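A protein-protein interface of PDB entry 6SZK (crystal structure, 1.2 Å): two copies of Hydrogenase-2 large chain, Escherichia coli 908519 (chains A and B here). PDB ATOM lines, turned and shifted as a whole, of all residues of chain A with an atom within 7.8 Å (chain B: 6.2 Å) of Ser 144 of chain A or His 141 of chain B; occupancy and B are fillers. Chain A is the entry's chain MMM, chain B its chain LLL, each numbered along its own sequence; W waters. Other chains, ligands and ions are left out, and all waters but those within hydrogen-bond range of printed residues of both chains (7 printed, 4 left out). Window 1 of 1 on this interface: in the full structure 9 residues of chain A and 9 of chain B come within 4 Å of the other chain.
The backbone carbonyl oxygen of His 141 of chain B lies within hydrogen-bond range of the side-chain hydroxyl of Ser 144 of chain A (3.3 Å).
The backbone carbonyl oxygen of His 141 of chain A is in hydrogen-bond range of the side-chain hydroxyl of Ser 144 of chain B (3.3 Å).
NZ of Lys 135 of chain B lies within salt-bridge range of OE2 of Glu 146 of chain A (2.9 Å).
A ring nitrogen (ND1) of His 141 of chain B is in hydrogen-bond range of the side-chain carboxylate of Glu 147 of chain A (2.8 Å).
NE2 of Gln 193 of chain A lies within hydrogen-bond range of O of Leu 142 of chain A (3.1 Å).
N of Glu 146 of chain B lies close to OG of Ser 144 of chain B (3.5 Å).
OG of Ser 144 of chain A is in hydrogen-bond range of N of Glu 147 of chain A (3.0 Å).
The backbone NH (N) of Trp 140 of chain B lies within hydrogen-bond range of the side-chain hydroxyl (OG) of Ser 138 of chain B.
OE2 of Glu 147 of chain A is in hydrogen-bond range of NE2 of Gln 193 of chain A, at 2.9 Å.
NE1 of Trp 140 of chain A is in hydrogen-bond range of OE1 of Gln 193 of chain A, at 2.9 Å.
Trp 140 of chain A touches Glu 146 of chain B.
Leu 142 of chain B touches His 141 of chain A.
CD2 of Leu 142 of chain A touches ND1 of His 141 of chain B (3.6 Å).
CD2 of Leu 142 of chain B touches CD2 of Leu 142 of chain A, at 3.6 Å.
CG of Pro 145 of chain A touches NZ of Lys 135 of chain B, 3.7 Å away.
Thr 139 of chain B touches Glu 146 of chain A (O to CB, 3.5 Å).
CB of Glu 146 of chain A touches O of Trp 140 of chain B, at 3.5 Å.
ND1 of His 141 of chain B touches CE of Lys 150 of chain A, 3.8 Å away.
Of the printed residues of chain B, Ser 144 of chain A touches His 141.
Printed residues of chain B within 4 Å of Glu 147 of chain A: His 141.
Of the printed residues of chain B, Lys 150 of chain A touches His 141 (3.8 Å).
Ala 189 of chain A touches none of the printed residues of chain B.
Of chain A, only Leu 142, Ser 144, Glu 147 and Lys 150 come within 4 Å of His 141 of chain B.
The nearest residue of chain B that does not touch Ser 144 of chain A is Ser 144 of chain B (4.2 Å).
The nearest residue of chain A that does not touch His 141 of chain B is Glu 146 of chain A (4.3 Å).
Hydrophobic or aromatic side chains of chain A within 4 Å of the printed part of chain B: His 141, Leu 142 and Pro 145.
Hydrophobic or aromatic side chains of chain B that line the printed part of chain A: His 141 and Leu 142.
Among the printed residues, Asp or Glu carboxylates within 4 Å of a Lys or Arg side-chain nitrogen of the other chain: Glu 146 of chain A with Lys 135 of chain B (2.9 Å).
Trp 140 of chain A touches Glu 146 of chain B, and with the chains exchanged Glu 146 of chain A touches Trp 140 of chain B.
His 141 of chain A touches Leu 142 of chain B, and with the chains exchanged Leu 142 of chain A touches His 141 of chain B.
His 141 of chain A touches Ser 144 of chain B, and with the chains exchanged Ser 144 of chain A touches His 141 of chain B.
Leu 142 of chain B touches its own counterpart, Leu 142 of chain A.
Positions printed for both chains: 140, 141, 142, 143, 144 and 146.
Water W1 lies within hydrogen-bond range of the side-chain carboxylate (OE1) of Glu 146 of chain A (2.7 Å) and the backbone carbonyl oxygen (O) of Asn 143 of chain B (3.3 Å).
Water W2 bridges OE2 of Glu 146 of chain B (2.7 Å) and O of Leu 134 of chain A (3.0 Å).
Water W7 lies within hydrogen-bond range of OE1 of Glu 146 of chain B (2.7 Å) and O of Asn 143 of chain A (3.4 Å).
Water W4 bridges the side-chain carboxylate (OE2) of Glu 146 of chain A (2.8 Å) and the backbone carbonyl oxygen (O) of Ser 138 of chain B (3.0 Å).
Water W3 lies within hydrogen-bond range of OE2 of Glu 147 of chain A, ND1 of His 141 of chain B and NZ of Lys 150 of chain A.
Water W6 lies within hydrogen-bond range of the backbone carbonyl oxygen of Glu 146 of chain A (2.8 Å) and the backbone carbonyl oxygen of Thr 139 of chain B (3.2 Å).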
ATOM      1  N   PRO A 127      -1.797  22.251   1.644  1.00  0.00           N
ATOM      2  CA  PRO A 127      -2.858  22.849   0.822  1.00  0.00           C
ATOM      3  C   PRO A 127      -2.597  24.277   0.330  1.00  0.00           C
ATOM      4  O   PRO A 127      -3.022  24.640  -0.799  1.00  0.00           O
ATOM      5  CB  PRO A 127      -4.142  22.707   1.677  1.00  0.00           C
ATOM      6  CG  PRO A 127      -3.854  21.461   2.510  1.00  0.00           C
ATOM      7  CD  PRO A 127      -2.368  21.649   2.867  1.00  0.00           C
ATOM      8  N   THR A 128      -1.954  25.114   1.172  1.00  0.00           N
ATOM      9  CA  THR A 128      -1.618  26.494   0.800  1.00  0.00           C
ATOM     10  C   THR A 128      -0.593  26.500  -0.339  1.00  0.00           C
ATOM     11  O   THR A 128      -0.771  27.285  -1.315  1.00  0.00           O
ATOM     12  CB  THR A 128      -1.156  27.297   2.024  1.00  0.00           C
ATOM     13  OG1 THR A 128      -2.252  27.330   2.967  1.00  0.00           O
ATOM     14  CG2 THR A 128      -0.754  28.698   1.645  1.00  0.00           C
ATOM     15  N   ALA A 130      -0.126  24.196  -2.527  1.00  0.00           N
ATOM     16  CA  ALA A 130      -0.832  23.639  -3.712  1.00  0.00           C
ATOM     17  C   ALA A 130      -1.627  24.759  -4.401  1.00  0.00           C
ATOM     18  O   ALA A 130      -1.541  24.944  -5.629  1.00  0.00           O
ATOM     19  CB  ALA A 130      -1.755  22.504  -3.277  1.00  0.00           C
ATOM     20  N   SER A 131      -2.394  25.553  -3.626  1.00  0.00           N
ATOM     21  CA  SER A 131      -3.161  26.671  -4.204  1.00  0.00           C
ATOM     22  C   SER A 131      -2.223  27.721  -4.838  1.00  0.00           C
ATOM     23  O   SER A 131      -2.461  28.205  -5.957  1.00  0.00           O
ATOM     24  CB  SER A 131      -4.049  27.267  -3.120  1.00  0.00           C
ATOM     25  OG  SER A 131      -4.830  28.341  -3.636  1.00  0.00           O
ATOM     26  N   GLU A 132      -1.076  27.991  -4.189  1.00  0.00           N
ATOM     27  CA  GLU A 132      -0.116  29.004  -4.723  1.00  0.00           C
ATOM     28  C   GLU A 132       0.440  28.582  -6.088  1.00  0.00           C
ATOM     29  O   GLU A 132       0.713  29.465  -6.920  1.00  0.00           O
ATOM     30  CB  GLU A 132       1.074  29.195  -3.764  1.00  0.00           C
ATOM     31  CG  GLU A 132       0.622  29.680  -2.432  1.00  0.00           C
ATOM     32  CD  GLU A 132       0.610  31.164  -2.262  1.00  0.00           C
ATOM     33  OE1 GLU A 132       0.507  31.572  -1.024  1.00  0.00           O
ATOM     34  OE2 GLU A 132       0.672  31.892  -3.350  1.00  0.00           O
ATOM     35  N   LEU A 134      -0.970  27.419  -8.576  1.00  0.00           N
ATOM     36  CA  LEU A 134      -1.938  27.682  -9.654  1.00  0.00           C
ATOM     37  C   LEU A 134      -2.132  29.183  -9.904  1.00  0.00           C
ATOM     38  O   LEU A 134      -2.853  29.510 -10.951  1.00  0.00           O
ATOM     39  CB  LEU A 134      -3.248  26.933  -9.380  1.00  0.00           C
ATOM     40  CG  LEU A 134      -3.161  25.407  -9.532  1.00  0.00           C
ATOM     41  CD1 LEU A 134      -4.405  24.716  -9.001  1.00  0.00           C
ATOM     42  CD2 LEU A 134      -2.806  24.894 -10.898  1.00  0.00           C
ATOM     43  N   TRP A 140      -9.823  29.531 -12.227  1.00  0.00           N
ATOM     44  CA  TRP A 140     -10.907  28.738 -11.605  1.00  0.00           C
ATOM     45  C   TRP A 140     -11.177  29.204 -10.163  1.00  0.00           C
ATOM     46  O   TRP A 140     -10.205  29.399  -9.365  1.00  0.00           O
ATOM     47  CB  TRP A 140     -10.526  27.252 -11.626  1.00  0.00           C
ATOM     48  CG  TRP A 140     -11.517  26.280 -11.020  1.00  0.00           C
ATOM     49  CD1 TRP A 140     -11.213  25.321 -10.095  1.00  0.00           C
ATOM     50  CD2 TRP A 140     -12.903  26.022 -11.365  1.00  0.00           C
ATOM     51  NE1 TRP A 140     -12.275  24.463  -9.848  1.00  0.00           N
ATOM     52  CE2 TRP A 140     -13.330  24.895 -10.606  1.00  0.00           C
ATOM     53  CE3 TRP A 140     -13.795  26.597 -12.315  1.00  0.00           C
ATOM     54  CZ2 TRP A 140     -14.628  24.369 -10.740  1.00  0.00           C
ATOM     55  CZ3 TRP A 140     -15.087  26.033 -12.441  1.00  0.00           C
ATOM     56  CH2 TRP A 140     -15.503  24.937 -11.671  1.00  0.00           C
ATOM     57  N   HIS A 141     -12.463  29.268  -9.810  1.00  0.00           N
ATOM     58  CA  HIS A 141     -12.902  29.789  -8.482  1.00  0.00           C
ATOM     59  C   HIS A 141     -12.832  28.740  -7.336  1.00  0.00           C
ATOM     60  O   HIS A 141     -13.117  29.169  -6.175  1.00  0.00           O
ATOM     61  CB  HIS A 141     -14.260  30.437  -8.577  1.00  0.00           C
ATOM     62  CG  HIS A 141     -15.420  29.488  -8.736  1.00  0.00           C
ATOM     63  ND1 HIS A 141     -16.697  29.856  -8.339  1.00  0.00           N
ATOM     64  CD2 HIS A 141     -15.589  28.237  -9.277  1.00  0.00           C
ATOM     65  CE1 HIS A 141     -17.545  28.865  -8.623  1.00  0.00           C
ATOM     66  NE2 HIS A 141     -16.897  27.844  -9.177  1.00  0.00           N
ATOM     67  N   LEU A 142     -12.475  27.444  -7.587  1.00  0.00           N
ATOM     68  CA  LEU A 142     -12.484  26.393  -6.539  1.00  0.00           C
ATOM     69  C   LEU A 142     -11.079  25.722  -6.378  1.00  0.00           C
ATOM     70  O   LEU A 142     -10.971  24.503  -6.250  1.00  0.00           O
ATOM     71  CB  LEU A 142     -13.603  25.392  -6.808  1.00  0.00           C
ATOM     72  CG  LEU A 142     -15.032  25.794  -6.338  1.00  0.00           C
ATOM     73  CD1 LEU A 142     -16.118  24.917  -6.914  1.00  0.00           C
ATOM     74  CD2 LEU A 142     -15.069  25.809  -4.815  1.00  0.00           C
ATOM     75  N   ASN A 143     -10.047  26.592  -6.389  1.00  0.00           N
ATOM     76  CA  ASN A 143      -8.634  26.213  -6.153  1.00  0.00           C
ATOM     77  C   ASN A 143      -8.075  26.751  -4.841  1.00  0.00           C
ATOM     78  O   ASN A 143      -6.858  26.793  -4.666  1.00  0.00           O
ATOM     79  CB  ASN A 143      -7.755  26.572  -7.328  1.00  0.00           C
ATOM     80  CG  ASN A 143      -7.878  25.647  -8.529  1.00  0.00           C
ATOM     81  OD1 ASN A 143      -8.170  24.442  -8.386  1.00  0.00           O
ATOM     82  ND2 ASN A 143      -7.645  26.218  -9.740  1.00  0.00           N
ATOM     83  N   SER A 144      -8.937  27.152  -3.886  1.00  0.00           N
ATOM     84  CA  SER A 144      -8.493  27.718  -2.596  1.00  0.00           C
ATOM     85  C   SER A 144      -7.806  26.679  -1.698  1.00  0.00           C
ATOM     86  O   SER A 144      -8.108  25.433  -1.743  1.00  0.00           O
ATOM     87  CB  SER A 144      -9.601  28.355  -1.826  1.00  0.00           C
ATOM     88  OG  SER A 144     -10.563  27.380  -1.422  1.00  0.00           O
ATOM     89  N   PRO A 145      -6.948  27.101  -0.739  1.00  0.00           N
ATOM     90  CA  PRO A 145      -6.442  26.188   0.323  1.00  0.00           C
ATOM     91  C   PRO A 145      -7.573  25.503   1.085  1.00  0.00           C
ATOM     92  O   PRO A 145      -7.422  24.341   1.495  1.00  0.00           O
ATOM     93  CB  PRO A 145      -5.493  27.038   1.193  1.00  0.00           C
ATOM     94  CG  PRO A 145      -5.170  28.244   0.318  1.00  0.00           C
ATOM     95  CD  PRO A 145      -6.397  28.460  -0.544  1.00  0.00           C
ATOM     96  N   GLU A 146      -8.656  26.251   1.334  1.00  0.00           N
ATOM     97  CA  GLU A 146      -9.831  25.699   2.088  1.00  0.00           C
ATOM     98  C   GLU A 146     -10.518  24.558   1.322  1.00  0.00           C
ATOM     99  O   GLU A 146     -10.859  23.543   1.960  1.00  0.00           O
ATOM    100  CB  GLU A 146     -10.749  26.895   2.414  1.00  0.00           C
ATOM    101  CG  GLU A 146     -10.220  27.924   3.387  1.00  0.00           C
ATOM    102  CD  GLU A 146      -9.137  28.866   2.860  1.00  0.00           C
ATOM    103  OE1 GLU A 146      -9.030  29.049   1.617  1.00  0.00           O
ATOM    104  OE2 GLU A 146      -8.469  29.567   3.704  1.00  0.00           O
ATOM    105  N   GLU A 147     -10.734  24.721   0.005  1.00  0.00           N
ATOM    106  CA  GLU A 147     -11.244  23.609  -0.801  1.00  0.00           C
ATOM    107  C   GLU A 147     -10.310  22.388  -0.712  1.00  0.00           C
ATOM    108  O   GLU A 147     -10.753  21.265  -0.526  1.00  0.00           O
ATOM    109  CB  GLU A 147     -11.420  24.086  -2.262  1.00  0.00           C
ATOM    110  CG  GLU A 147     -11.871  22.955  -3.231  1.00  0.00           C
ATOM    111  CD  GLU A 147     -13.322  22.507  -3.132  1.00  0.00           C
ATOM    112  OE1 GLU A 147     -14.070  22.973  -2.175  1.00  0.00           O
ATOM    113  OE2 GLU A 147     -13.766  21.713  -4.008  1.00  0.00           O
ATOM    114  N   PHE A 148      -9.008  22.625  -0.903  1.00  0.00           N
ATOM    115  CA  PHE A 148      -8.012  21.545  -0.937  1.00  0.00           C
ATOM    116  C   PHE A 148      -7.921  20.844   0.442  1.00  0.00           C
ATOM    117  O   PHE A 148      -7.716  19.605   0.502  1.00  0.00           O
ATOM    118  CB  PHE A 148      -6.667  22.017  -1.482  1.00  0.00           C
ATOM    119  CG  PHE A 148      -6.633  22.471  -2.919  1.00  0.00           C
ATOM    120  CD1 PHE A 148      -7.624  22.149  -3.825  1.00  0.00           C
ATOM    121  CD2 PHE A 148      -5.571  23.226  -3.361  1.00  0.00           C
ATOM    122  CE1 PHE A 148      -7.545  22.554  -5.149  1.00  0.00           C
ATOM    123  CE2 PHE A 148      -5.465  23.606  -4.689  1.00  0.00           C
ATOM    124  CZ  PHE A 148      -6.463  23.295  -5.609  1.00  0.00           C
ATOM    125  N   THR A 149      -8.080  21.610   1.551  1.00  0.00           N
ATOM    126  CA  THR A 149      -8.049  21.005   2.916  1.00  0.00           C
ATOM    127  C   THR A 149      -9.281  20.104   3.109  1.00  0.00           C
ATOM    128  O   THR A 149      -9.168  18.998   3.647  1.00  0.00           O
ATOM    129  CB  THR A 149      -7.974  22.103   3.987  1.00  0.00           C
ATOM    130  OG1 THR A 149      -6.769  22.851   3.807  1.00  0.00           O
ATOM    131  CG2 THR A 149      -8.015  21.543   5.393  1.00  0.00           C
ATOM    132  N   LYS A 150     -10.458  20.550   2.646  1.00  0.00           N
ATOM    133  CA  LYS A 150     -11.689  19.714   2.773  1.00  0.00           C
ATOM    134  C   LYS A 150     -11.482  18.384   2.004  1.00  0.00           C
ATOM    135  O   LYS A 150     -11.889  17.290   2.510  1.00  0.00           O
ATOM    136  CB  LYS A 150     -12.907  20.517   2.235  1.00  0.00           C
ATOM    137  CG  LYS A 150     -14.260  19.862   2.174  1.00  0.00           C
ATOM    138  CD  LYS A 150     -15.395  20.767   1.590  1.00  0.00           C
ATOM    139  CE  LYS A 150     -15.074  21.466   0.260  1.00  0.00           C
ATOM    140  NZ  LYS A 150     -15.547  20.699  -0.896  1.00  0.00           N
ATOM    141  N   LEU A 185      -2.854  16.260  -4.759  1.00  0.00           N
ATOM    142  CA  LEU A 185      -4.045  16.775  -4.040  1.00  0.00           C
ATOM    143  C   LEU A 185      -4.899  17.627  -4.996  1.00  0.00           C
ATOM    144  O   LEU A 185      -6.147  17.456  -4.980  1.00  0.00           O
ATOM    145  CB  LEU A 185      -3.633  17.528  -2.771  1.00  0.00           C
ATOM    146  CG  LEU A 185      -4.775  18.190  -2.009  1.00  0.00           C
ATOM    147  CD1 LEU A 185      -5.821  17.164  -1.530  1.00  0.00           C
ATOM    148  CD2 LEU A 185      -4.241  19.004  -0.803  1.00  0.00           C
ATOM    149  N   ALA A 189      -8.999  16.888  -5.969  1.00  0.00           N
ATOM    150  CA  ALA A 189     -10.044  17.940  -5.897  1.00  0.00           C
ATOM    151  C   ALA A 189     -10.762  18.112  -7.252  1.00  0.00           C
ATOM    152  O   ALA A 189     -11.997  18.211  -7.271  1.00  0.00           O
ATOM    153  CB  ALA A 189      -9.433  19.261  -5.446  1.00  0.00           C
ATOM    154  N   GLN A 193     -14.750  17.598  -8.527  1.00  0.00           N
ATOM    155  CA  GLN A 193     -15.469  18.743  -9.191  1.00  0.00           C
ATOM    156  C   GLN A 193     -15.978  18.338 -10.590  1.00  0.00           C
ATOM    157  O   GLN A 193     -17.056  18.816 -11.064  1.00  0.00           O
ATOM    158  CB  GLN A 193     -14.547  19.982  -9.252  1.00  0.00           C
ATOM    159  CG  GLN A 193     -14.207  20.571  -7.876  1.00  0.00           C
ATOM    160  CD  GLN A 193     -13.005  21.491  -7.858  1.00  0.00           C
ATOM    161  OE1 GLN A 193     -12.432  21.770  -8.907  1.00  0.00           O
ATOM    162  NE2 GLN A 193     -12.542  21.893  -6.652  1.00  0.00           N
ATOM    163  N   GLU A 196     -19.646  17.070 -10.953  1.00  0.00           N
ATOM    164  CA  GLU A 196     -20.726  18.091 -11.091  1.00  0.00           C
ATOM    165  C   GLU A 196     -20.845  18.583 -12.543  1.00  0.00           C
ATOM    166  O   GLU A 196     -21.982  18.727 -13.095  1.00  0.00           O
ATOM    167  CB  GLU A 196     -20.516  19.300 -10.152  1.00  0.00           C
ATOM    168  CG  GLU A 196     -21.719  20.279 -10.125  1.00  0.00           C
ATOM    169  CD  GLU A 196     -21.652  21.524  -9.231  1.00  0.00           C
ATOM    170  OE1 GLU A 196     -20.790  21.535  -8.319  1.00  0.00           O
ATOM    171  OE2 GLU A 196     -22.427  22.541  -9.450  1.00  0.00           O
ATOM    172  N   LYS B 135      -8.180  34.459   6.244  1.00  0.00           N
ATOM    173  CA  LYS B 135      -7.339  33.281   6.673  1.00  0.00           C
ATOM    174  C   LYS B 135      -7.378  33.122   8.184  1.00  0.00           C
ATOM    175  O   LYS B 135      -7.061  34.134   8.821  1.00  0.00           O
ATOM    176  CB  LYS B 135      -5.866  33.454   6.356  1.00  0.00           C
ATOM    177  CG  LYS B 135      -5.653  33.602   4.909  1.00  0.00           C
ATOM    178  CD  LYS B 135      -5.979  32.276   4.239  1.00  0.00           C
ATOM    179  CE  LYS B 135      -6.107  32.407   2.735  1.00  0.00           C
ATOM    180  NZ  LYS B 135      -6.498  31.118   2.190  1.00  0.00           N
ATOM    181  N   SER B 138     -12.454  31.991   8.608  1.00  0.00           N
ATOM    182  CA  SER B 138     -13.437  31.091   7.985  1.00  0.00           C
ATOM    183  C   SER B 138     -12.724  29.927   7.284  1.00  0.00           C
ATOM    184  O   SER B 138     -11.617  30.170   6.708  1.00  0.00           O
ATOM    185  CB  SER B 138     -14.254  31.834   6.970  1.00  0.00           C
ATOM    186  OG  SER B 138     -15.162  30.968   6.300  1.00  0.00           O
ATOM    187  N   THR B 139     -13.382  28.773   7.191  1.00  0.00           N
ATOM    188  CA  THR B 139     -12.973  27.631   6.380  1.00  0.00           C
ATOM    189  C   THR B 139     -13.828  27.493   5.094  1.00  0.00           C
ATOM    190  O   THR B 139     -13.666  26.468   4.371  1.00  0.00           O
ATOM    191  CB  THR B 139     -13.027  26.322   7.211  1.00  0.00           C
ATOM    192  OG1 THR B 139     -14.395  26.027   7.523  1.00  0.00           O
ATOM    193  CG2 THR B 139     -12.124  26.303   8.439  1.00  0.00           C
ATOM    194  N   TRP B 140     -14.659  28.515   4.766  1.00  0.00           N
ATOM    195  CA  TRP B 140     -15.502  28.443   3.539  1.00  0.00           C
ATOM    196  C   TRP B 140     -14.652  28.251   2.266  1.00  0.00           C
ATOM    197  O   TRP B 140     -13.590  28.910   2.157  1.00  0.00           O
ATOM    198  CB  TRP B 140     -16.323  29.724   3.443  1.00  0.00           C
ATOM    199  CG  TRP B 140     -17.215  29.875   2.243  1.00  0.00           C
ATOM    200  CD1 TRP B 140     -17.235  30.945   1.393  1.00  0.00           C
ATOM    201  CD2 TRP B 140     -18.348  29.047   1.826  1.00  0.00           C
ATOM    202  NE1 TRP B 140     -18.285  30.869   0.505  1.00  0.00           N
ATOM    203  CE2 TRP B 140     -18.986  29.705   0.732  1.00  0.00           C
ATOM    204  CE3 TRP B 140     -18.901  27.841   2.314  1.00  0.00           C
ATOM    205  CZ2 TRP B 140     -20.138  29.179   0.105  1.00  0.00           C
ATOM    206  CZ3 TRP B 140     -20.024  27.324   1.712  1.00  0.00           C
ATOM    207  CH2 TRP B 140     -20.658  27.986   0.634  1.00  0.00           C
ATOM    208  N   HIS B 141     -15.121  27.392   1.366  1.00  0.00           N
ATOM    209  CA  HIS B 141     -14.372  27.022   0.138  1.00  0.00           C
ATOM    210  C   HIS B 141     -14.481  28.043  -1.020  1.00  0.00           C
ATOM    211  O   HIS B 141     -13.810  27.804  -2.037  1.00  0.00           O
ATOM    212  CB  HIS B 141     -14.751  25.608  -0.294  1.00  0.00           C
ATOM    213  CG  HIS B 141     -16.115  25.449  -0.915  1.00  0.00           C
ATOM    214  ND1 HIS B 141     -16.386  24.407  -1.776  1.00  0.00           N
ATOM    215  CD2 HIS B 141     -17.272  26.155  -0.772  1.00  0.00           C
ATOM    216  CE1 HIS B 141     -17.671  24.482  -2.228  1.00  0.00           C
ATOM    217  NE2 HIS B 141     -18.259  25.548  -1.608  1.00  0.00           N
ATOM    218  N   LEU B 142     -15.280  29.110  -0.891  1.00  0.00           N
ATOM    219  CA  LEU B 142     -15.504  30.085  -1.986  1.00  0.00           C
ATOM    220  C   LEU B 142     -15.120  31.551  -1.592  1.00  0.00           C
ATOM    221  O   LEU B 142     -15.833  32.530  -1.955  1.00  0.00           O
ATOM    222  CB  LEU B 142     -16.951  29.977  -2.530  1.00  0.00           C
ATOM    223  CG  LEU B 142     -17.191  28.843  -3.520  1.00  0.00           C
ATOM    224  CD1 LEU B 142     -18.697  28.587  -3.699  1.00  0.00           C
ATOM    225  CD2 LEU B 142     -16.515  29.131  -4.871  1.00  0.00           C
ATOM    226  N   ASN B 143     -13.967  31.672  -0.952  1.00  0.00           N
ATOM    227  CA  ASN B 143     -13.353  32.965  -0.549  1.00  0.00           C
ATOM    228  C   ASN B 143     -12.026  33.229  -1.264  1.00  0.00           C
ATOM    229  O   ASN B 143     -11.205  34.050  -0.786  1.00  0.00           O
ATOM    230  CB  ASN B 143     -13.165  33.052   0.988  1.00  0.00           C
ATOM    231  CG  ASN B 143     -14.437  33.285   1.808  1.00  0.00           C
ATOM    232  OD1 ASN B 143     -14.511  32.858   3.010  1.00  0.00           O
ATOM    233  ND2 ASN B 143     -15.361  33.990   1.223  1.00  0.00           N
ATOM    234  N   SER B 144     -11.770  32.573  -2.427  1.00  0.00           N
ATOM    235  CA  SER B 144     -10.484  32.763  -3.142  1.00  0.00           C
ATOM    236  C   SER B 144     -10.429  34.148  -3.801  1.00  0.00           C
ATOM    237  O   SER B 144     -11.464  34.767  -4.170  1.00  0.00           O
ATOM    238  CB  SER B 144     -10.288  31.687  -4.222  1.00  0.00           C
ATOM    239  OG  SER B 144     -11.318  31.810  -5.250  1.00  0.00           O
ATOM    240  N   GLU B 146      -9.745  34.466  -6.859  1.00  0.00           N
ATOM    241  CA  GLU B 146     -10.346  34.218  -8.178  1.00  0.00           C
ATOM    242  C   GLU B 146     -11.892  34.395  -8.112  1.00  0.00           C
ATOM    243  O   GLU B 146     -12.461  35.040  -9.026  1.00  0.00           O
ATOM    244  CB  GLU B 146      -9.933  32.834  -8.727  1.00  0.00           C
ATOM    245  CG  GLU B 146      -8.482  32.705  -9.098  1.00  0.00           C
ATOM    246  CD  GLU B 146      -7.490  32.590  -7.947  1.00  0.00           C
ATOM    247  OE1 GLU B 146      -7.894  32.346  -6.783  1.00  0.00           O
ATOM    248  OE2 GLU B 146      -6.233  32.741  -8.198  1.00  0.00           O
ATOM    249  N   GLN B 256     -20.116  28.929   7.986  1.00  0.00           N
ATOM    250  CA  GLN B 256     -18.803  29.442   7.551  1.00  0.00           C
ATOM    251  C   GLN B 256     -18.896  30.808   6.831  1.00  0.00           C
ATOM    252  O   GLN B 256     -17.856  31.462   6.557  1.00  0.00           O
ATOM    253  CB  GLN B 256     -18.081  28.423   6.629  1.00  0.00           C
ATOM    254  CG  GLN B 256     -17.916  27.013   7.230  1.00  0.00           C
ATOM    255  CD  GLN B 256     -17.611  25.896   6.202  1.00  0.00           C
ATOM    256  OE1 GLN B 256     -17.384  26.114   4.981  1.00  0.00           O
ATOM    257  NE2 GLN B 256     -17.565  24.640   6.681  1.00  0.00           N
HETATM  258  O   HOH W   1      -9.722  31.284   0.360  1.00  0.00           O
HETATM  259  O   HOH W   2      -5.127  30.605  -9.353  1.00  0.00           O
HETATM  260  O   HOH W   3     -16.513  22.003  -3.996  1.00  0.00           O
HETATM  261  O   HOH W   4      -9.946  31.681   4.691  1.00  0.00           O
HETATM  262  O   HOH W   5      -8.993  29.713   6.635  1.00  0.00           O
HETATM  263  O   HOH W   6     -11.665  24.014   4.571  1.00  0.00           O
HETATM  264  O   HOH W   7      -7.323  30.009  -5.521  1.00  0.00           O
